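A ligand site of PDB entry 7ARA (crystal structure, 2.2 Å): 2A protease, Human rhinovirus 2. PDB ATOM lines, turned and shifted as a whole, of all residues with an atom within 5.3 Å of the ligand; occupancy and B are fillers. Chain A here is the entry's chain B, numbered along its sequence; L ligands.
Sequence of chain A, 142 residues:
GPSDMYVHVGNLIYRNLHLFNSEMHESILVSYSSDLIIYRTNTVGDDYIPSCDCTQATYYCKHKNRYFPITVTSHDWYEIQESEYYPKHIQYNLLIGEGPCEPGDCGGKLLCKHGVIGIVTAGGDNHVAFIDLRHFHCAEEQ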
ATOM      1  N   HIS A  18      25.324  26.226   8.403  1.00  0.00           N
ATOM      2  CA  HIS A  18      25.773  25.333   7.328  1.00  0.00           C
ATOM      3  C   HIS A  18      25.790  26.028   5.960  1.00  0.00           C
ATOM      4  O   HIS A  18      26.312  25.472   4.992  1.00  0.00           O
ATOM      5  CB  HIS A  18      24.908  24.073   7.281  1.00  0.00           C
ATOM      6  CG  HIS A  18      23.439  24.345   7.132  1.00  0.00           C
ATOM      7  ND1 HIS A  18      22.896  24.935   6.013  1.00  0.00           N
ATOM      8  CD2 HIS A  18      22.412  24.084   7.964  1.00  0.00           C
ATOM      9  CE1 HIS A  18      21.587  25.033   6.166  1.00  0.00           C
ATOM     10  NE2 HIS A  18      21.270  24.525   7.341  1.00  0.00           N
ATOM     11  N   LEU A  19      25.214  27.223   5.892  1.00  0.00           N
ATOM     12  CA  LEU A  19      25.252  28.018   4.660  1.00  0.00           C
ATOM     13  C   LEU A  19      26.541  28.840   4.586  1.00  0.00           C
ATOM     14  O   LEU A  19      26.659  29.745   3.761  1.00  0.00           O
ATOM     15  CB  LEU A  19      24.044  28.958   4.585  1.00  0.00           C
ATOM     16  CG  LEU A  19      22.646  28.388   4.335  1.00  0.00           C
ATOM     17  CD1 LEU A  19      21.768  29.462   3.694  1.00  0.00           C
ATOM     18  CD2 LEU A  19      22.674  27.132   3.481  1.00  0.00           C
ATOM     19  N   TYR A  78      14.115  22.481  22.237  1.00  0.00           N
ATOM     20  CA  TYR A  78      13.357  21.502  21.466  1.00  0.00           C
ATOM     21  C   TYR A  78      14.306  20.461  20.886  1.00  0.00           C
ATOM     22  O   TYR A  78      15.390  20.790  20.395  1.00  0.00           O
ATOM     23  CB  TYR A  78      12.554  22.182  20.355  1.00  0.00           C
ATOM     24  CG  TYR A  78      11.425  21.347  19.775  1.00  0.00           C
ATOM     25  CD1 TYR A  78      11.687  20.310  18.883  1.00  0.00           C
ATOM     26  CD2 TYR A  78      10.105  21.602  20.120  1.00  0.00           C
ATOM     27  CE1 TYR A  78      10.663  19.552  18.342  1.00  0.00           C
ATOM     28  CE2 TYR A  78       9.071  20.845  19.589  1.00  0.00           C
ATOM     29  CZ  TYR A  78       9.355  19.825  18.700  1.00  0.00           C
ATOM     30  OH  TYR A  78       8.333  19.063  18.172  1.00  0.00           O
ATOM     31  N   GLU A  79      13.877  19.198  20.940  1.00  0.00           N
ATOM     32  CA  GLU A  79      14.686  18.114  20.385  1.00  0.00           C
ATOM     33  C   GLU A  79      14.619  18.143  18.868  1.00  0.00           C
ATOM     34  O   GLU A  79      13.604  17.746  18.282  1.00  0.00           O
ATOM     35  CB  GLU A  79      14.193  16.758  20.908  1.00  0.00           C
ATOM     36  CG  GLU A  79      15.109  15.596  20.546  1.00  0.00           C
ATOM     37  CD  GLU A  79      14.974  14.423  21.498  1.00  0.00           C
ATOM     38  OE1 GLU A  79      13.824  13.999  21.769  1.00  0.00           O
ATOM     39  OE2 GLU A  79      16.015  13.909  21.969  1.00  0.00           O
ATOM     40  N   ILE A  80      15.681  18.625  18.256  1.00  0.00           N
ATOM     41  CA  ILE A  80      15.760  18.597  16.811  1.00  0.00           C
ATOM     42  C   ILE A  80      16.494  17.303  16.421  1.00  0.00           C
ATOM     43  O   ILE A  80      17.665  17.101  16.751  1.00  0.00           O
ATOM     44  CB  ILE A  80      16.436  19.894  16.232  1.00  0.00           C
ATOM     45  CG1 ILE A  80      16.162  20.033  14.740  1.00  0.00           C
ATOM     46  CG2 ILE A  80      17.916  19.994  16.563  1.00  0.00           C
ATOM     47  CD1 ILE A  80      14.802  20.634  14.438  1.00  0.00           C
ATOM     48  N   GLN A  81      15.763  16.394  15.774  1.00  0.00           N
ATOM     49  CA  GLN A  81      16.287  15.069  15.469  1.00  0.00           C
ATOM     50  C   GLN A  81      17.377  15.107  14.412  1.00  0.00           C
ATOM     51  O   GLN A  81      17.875  16.180  14.053  1.00  0.00           O
ATOM     52  CB  GLN A  81      15.157  14.133  15.033  1.00  0.00           C
ATOM     53  N   GLU A  82      17.753  13.942  13.907  1.00  0.00           N
ATOM     54  CA  GLU A  82      18.872  13.830  12.978  1.00  0.00           C
ATOM     55  C   GLU A  82      18.448  13.620  11.530  1.00  0.00           C
ATOM     56  O   GLU A  82      17.728  12.676  11.220  1.00  0.00           O
ATOM     57  CB  GLU A  82      19.794  12.678  13.407  1.00  0.00           C
ATOM     58  N   SER A  83      18.906  14.515  10.663  1.00  0.00           N
ATOM     59  CA  SER A  83      18.848  14.311   9.214  1.00  0.00           C
ATOM     60  C   SER A  83      20.208  13.810   8.736  1.00  0.00           C
ATOM     61  O   SER A  83      21.125  13.617   9.548  1.00  0.00           O
ATOM     62  CB  SER A  83      18.444  15.609   8.498  1.00  0.00           C
ATOM     63  OG  SER A  83      18.949  16.749   9.174  1.00  0.00           O
ATOM     64  N   LEU A  94      13.681  28.466  19.790  1.00  0.00           N
ATOM     65  CA  LEU A  94      13.075  28.210  18.501  1.00  0.00           C
ATOM     66  C   LEU A  94      11.750  28.923  18.361  1.00  0.00           C
ATOM     67  O   LEU A  94      11.130  29.304  19.358  1.00  0.00           O
ATOM     68  CB  LEU A  94      12.886  26.709  18.285  1.00  0.00           C
ATOM     69  CG  LEU A  94      14.063  25.966  17.668  1.00  0.00           C
ATOM     70  CD1 LEU A  94      13.771  24.485  17.634  1.00  0.00           C
ATOM     71  CD2 LEU A  94      14.331  26.504  16.274  1.00  0.00           C
ATOM     72  N   ILE A  96       8.041  28.166  16.290  1.00  0.00           N
ATOM     73  CA  ILE A  96       7.336  27.153  15.507  1.00  0.00           C
ATOM     74  C   ILE A  96       5.880  27.519  15.218  1.00  0.00           C
ATOM     75  O   ILE A  96       5.127  27.898  16.117  1.00  0.00           O
ATOM     76  CB  ILE A  96       7.364  25.782  16.207  1.00  0.00           C
ATOM     77  CG1 ILE A  96       8.799  25.268  16.288  1.00  0.00           C
ATOM     78  CG2 ILE A  96       6.511  24.784  15.457  1.00  0.00           C
ATOM     79  CD1 ILE A  96       9.217  24.853  17.684  1.00  0.00           C
ATOM     80  N   CYS A 101       7.578  23.141   4.245  1.00  0.00           N
ATOM     81  CA  CYS A 101       9.027  23.171   4.307  1.00  0.00           C
ATOM     82  C   CYS A 101       9.637  22.084   3.441  1.00  0.00           C
ATOM     83  O   CYS A 101       9.155  20.952   3.392  1.00  0.00           O
ATOM     84  CB  CYS A 101       9.494  23.017   5.753  1.00  0.00           C
ATOM     85  SG  CYS A 101      11.228  23.488   5.995  1.00  0.00           S
ATOM     86  N   GLU A 102      10.728  22.444   2.762  1.00  0.00           N
ATOM     87  CA  GLU A 102      11.419  21.562   1.835  1.00  0.00           C
ATOM     88  C   GLU A 102      12.884  21.983   1.772  1.00  0.00           C
ATOM     89  O   GLU A 102      13.186  23.164   1.902  1.00  0.00           O
ATOM     90  CB  GLU A 102      10.750  21.617   0.454  1.00  0.00           C
ATOM     91  CG  GLU A 102      11.387  20.767  -0.621  1.00  0.00           C
ATOM     92  CD  GLU A 102      10.351  20.082  -1.492  1.00  0.00           C
ATOM     93  OE1 GLU A 102       9.202  19.922  -1.033  1.00  0.00           O
ATOM     94  OE2 GLU A 102      10.692  19.715  -2.637  1.00  0.00           O
ATOM     95  N   PRO A 103      13.806  21.010   1.621  1.00  0.00           N
ATOM     96  CA  PRO A 103      15.239  21.301   1.519  1.00  0.00           C
ATOM     97  C   PRO A 103      15.595  22.476   0.615  1.00  0.00           C
ATOM     98  O   PRO A 103      15.086  22.583  -0.500  1.00  0.00           O
ATOM     99  CB  PRO A 103      15.810  20.000   0.965  1.00  0.00           C
ATOM    100  CG  PRO A 103      14.953  18.958   1.568  1.00  0.00           C
ATOM    101  CD  PRO A 103      13.558  19.560   1.676  1.00  0.00           C
ATOM    102  N   GLY A 104      16.463  23.346   1.121  1.00  0.00           N
ATOM    103  CA  GLY A 104      16.873  24.530   0.397  1.00  0.00           C
ATOM    104  C   GLY A 104      16.120  25.766   0.843  1.00  0.00           C
ATOM    105  O   GLY A 104      16.218  26.823   0.233  1.00  0.00           O
ATOM    106  N   ASP A 105      15.353  25.641   1.930  1.00  0.00           N
ATOM    107  CA  ASP A 105      14.515  26.737   2.386  1.00  0.00           C
ATOM    108  C   ASP A 105      15.100  27.493   3.574  1.00  0.00           C
ATOM    109  O   ASP A 105      14.514  28.471   4.035  1.00  0.00           O
ATOM    110  CB  ASP A 105      13.118  26.222   2.747  1.00  0.00           C
ATOM    111  CG  ASP A 105      12.251  25.970   1.525  1.00  0.00           C
ATOM    112  OD1 ASP A 105      12.818  25.729   0.437  1.00  0.00           O
ATOM    113  OD2 ASP A 105      11.001  26.005   1.653  1.00  0.00           O
ATOM    114  N   CYS A 106      16.251  27.041   4.070  1.00  0.00           N
ATOM    115  CA  CYS A 106      16.865  27.706   5.211  1.00  0.00           C
ATOM    116  C   CYS A 106      17.339  29.092   4.848  1.00  0.00           C
ATOM    117  O   CYS A 106      17.881  29.309   3.766  1.00  0.00           O
ATOM    118  CB  CYS A 106      18.037  26.891   5.753  1.00  0.00           C
ATOM    119  SG  CYS A 106      17.668  25.166   6.001  1.00  0.00           S
ATOM    120  N   THR A 121      15.281  27.290   9.875  1.00  0.00           N
ATOM    121  CA  THR A 121      16.436  26.434  10.196  1.00  0.00           C
ATOM    122  C   THR A 121      16.134  24.967   9.977  1.00  0.00           C
ATOM    123  O   THR A 121      17.020  24.180   9.643  1.00  0.00           O
ATOM    124  CB  THR A 121      16.903  26.627  11.662  1.00  0.00           C
ATOM    125  OG1 THR A 121      17.939  25.672  11.961  1.00  0.00           O
ATOM    126  CG2 THR A 121      15.747  26.456  12.630  1.00  0.00           C
ATOM    127  N   ALA A 122      14.867  24.601  10.165  1.00  0.00           N
ATOM    128  CA  ALA A 122      14.416  23.227   9.964  1.00  0.00           C
ATOM    129  C   ALA A 122      12.902  23.173   9.870  1.00  0.00           C
ATOM    130  O   ALA A 122      12.205  24.112  10.262  1.00  0.00           O
ATOM    131  CB  ALA A 122      14.908  22.327  11.099  1.00  0.00           C
ATOM    132  N   GLY A 123      12.388  22.062   9.344  1.00  0.00           N
ATOM    133  CA  GLY A 123      10.962  21.855   9.233  1.00  0.00           C
ATOM    134  C   GLY A 123      10.593  20.381   9.143  1.00  0.00           C
ATOM    135  O   GLY A 123      11.456  19.512   9.185  1.00  0.00           O
ATOM    136  N   GLY A 124       9.303  20.110   9.019  1.00  0.00           N
ATOM    137  CA  GLY A 124       8.825  18.745   8.894  1.00  0.00           C
ATOM    138  C   GLY A 124       7.537  18.693   8.113  1.00  0.00           C
ATOM    139  O   GLY A 124       7.270  19.528   7.250  1.00  0.00           O
ATOM    140  N   HIS A 127       4.993  21.571   9.311  1.00  0.00           N
ATOM    141  CA  HIS A 127       5.433  22.439  10.401  1.00  0.00           C
ATOM    142  C   HIS A 127       6.870  22.896  10.166  1.00  0.00           C
ATOM    143  O   HIS A 127       7.720  22.098   9.770  1.00  0.00           O
ATOM    144  CB  HIS A 127       5.339  21.720  11.748  1.00  0.00           C
ATOM    145  CG  HIS A 127       3.955  21.657  12.299  1.00  0.00           C
ATOM    146  ND1 HIS A 127       3.087  20.620  12.018  1.00  0.00           N
ATOM    147  CD2 HIS A 127       3.273  22.497  13.131  1.00  0.00           C
ATOM    148  CE1 HIS A 127       1.935  20.829  12.644  1.00  0.00           C
ATOM    149  NE2 HIS A 127       2.028  21.954  13.323  1.00  0.00           N
ATOM    150  N   VAL A 128       7.127  24.177  10.409  1.00  0.00           N
ATOM    151  CA  VAL A 128       8.427  24.765  10.105  1.00  0.00           C
ATOM    152  C   VAL A 128       8.991  25.508  11.314  1.00  0.00           C
ATOM    153  O   VAL A 128       8.248  26.145  12.069  1.00  0.00           O
ATOM    154  CB  VAL A 128       8.318  25.701   8.879  1.00  0.00           C
ATOM    155  CG1 VAL A 128       7.265  26.784   9.122  1.00  0.00           C
ATOM    156  CG2 VAL A 128       9.665  26.316   8.541  1.00  0.00           C
ATOM    157  N   ALA A 129      10.315  25.417  11.499  1.00  0.00           N
ATOM    158  CA  ALA A 129      10.976  26.011  12.668  1.00  0.00           C
ATOM    159  C   ALA A 129      11.934  27.135  12.283  1.00  0.00           C
ATOM    160  O   ALA A 129      12.627  27.057  11.264  1.00  0.00           O
ATOM    161  CB  ALA A 129      11.717  24.940  13.443  1.00  0.00           C
HETATM  162  C1  LIG L   1      16.604  18.676   7.135  1.00  0.00           C
HETATM  163  C2  LIG L   1       9.581  20.464  13.557  1.00  0.00           C
HETATM  164  C3  LIG L   1       8.235  20.820  13.769  1.00  0.00           C
HETATM  165  C4  LIG L   1       7.885  21.551  14.913  1.00  0.00           C
HETATM  166  C5  LIG L   1      10.219  21.552  15.602  1.00  0.00           C
HETATM  167  C6  LIG L   1      15.407  17.522  11.557  1.00  0.00           C
HETATM  168  C7  LIG L   1      16.812  18.070  11.805  1.00  0.00           C
HETATM  169  C8  LIG L   1      12.526  20.135   6.370  1.00  0.00           C
HETATM  170  C9  LIG L   1      14.414  22.095   5.414  1.00  0.00           C
HETATM  171  C10 LIG L   1      15.833  21.587   5.047  1.00  0.00           C
HETATM  172  C11 LIG L   1      16.872  22.527   5.658  1.00  0.00           C
HETATM  173  C12 LIG L   1      17.346  20.996   7.865  1.00  0.00           C
HETATM  174  C13 LIG L   1      16.171  19.948   7.858  1.00  0.00           C
HETATM  175  C14 LIG L   1      14.728  18.860   9.601  1.00  0.00           C
HETATM  176  C15 LIG L   1      14.445  18.579  11.089  1.00  0.00           C
HETATM  177  C16 LIG L   1      12.146  18.571  12.320  1.00  0.00           C
HETATM  178  C17 LIG L   1       9.989  19.660  12.323  1.00  0.00           C
HETATM  179  C18 LIG L   1       8.867  21.914  15.818  1.00  0.00           C
HETATM  180  C19 LIG L   1      10.559  20.821  14.468  1.00  0.00           C
HETATM  181  C20 LIG L   1      14.860  16.775  12.785  1.00  0.00           C
HETATM  182  C21 LIG L   1      17.907  22.920   4.602  1.00  0.00           C
HETATM  183  C22 LIG L   1      18.526  24.313   4.704  1.00  0.00           C
HETATM  184  N1  LIG L   1      17.591  22.077   6.862  1.00  0.00           N
HETATM  185  N2  LIG L   1      15.841  19.670   9.240  1.00  0.00           N
HETATM  186  N3  LIG L   1      13.059  18.092  11.246  1.00  0.00           N
HETATM  187  O1  LIG L   1      18.158  20.889   8.778  1.00  0.00           O
HETATM  188  O2  LIG L   1      14.003  18.373   8.750  1.00  0.00           O
HETATM  189  O3  LIG L   1      11.996  17.910  13.352  1.00  0.00           O
HETATM  190  O4  LIG L   1      11.420  19.816  12.185  1.00  0.00           O
HETATM  191  O5  LIG L   1      18.223  22.159   3.711  1.00  0.00           O
HETATM  192  S1  LIG L   1      13.244  20.880   4.897  1.00  0.00           S
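O of Ala 122 sits at hydrogen-bond distance from N of Ala 129. The backbone carbonyl oxygen (O) of Ala 129 sits at hydrogen-bond distance from the backbone NH (N) of Thr 121 (3.0 Å).
SG of Cys 101 sits close to S1 of the ligand, 3.5 Å away. A nitrogen (N3) of the ligand sits at hydrogen-bond distance from the backbone carbonyl oxygen of Gly 123 (3.0 Å). The backbone NH (N) of Glu 102 lies close to a sulfur (S1) of the ligand (3.7 Å). An oxygen (O5) of the ligand sits at hydrogen-bond distance from the backbone NH (N) of Gly 104, 3.3 Å away. SG of Cys 106 is covalently linked to C22 of the ligand, 1.8 Å away.
N of Pro 103 sits close to S1 of the ligand. His 18 touches the ligand. Tyr 78 touches the ligand. Ile 80 touches the ligand. Gln 81 touches the ligand. Ser 83 touches the ligand. Ile 96 touches the ligand. Thr 121 touches the ligand (O to N1, 3.5 Å). Ala 122 touches the ligand. Gly 124 touches the ligand (N to C17, 3.4 Å). His 127 touches the ligand (CB to C3, 3.6 Å). Hydrophobic or aromatic side chains within 4 Å of the ligand: His 18, Tyr 78, Ile 80, Ile 96, Pro 103, Ala 122 and His 127. Of the 23 residues printed, 16 come within 4 Å of the ligand. The nearest printed residue that does not touch the ligand is Glu 82 (4.2 Å).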
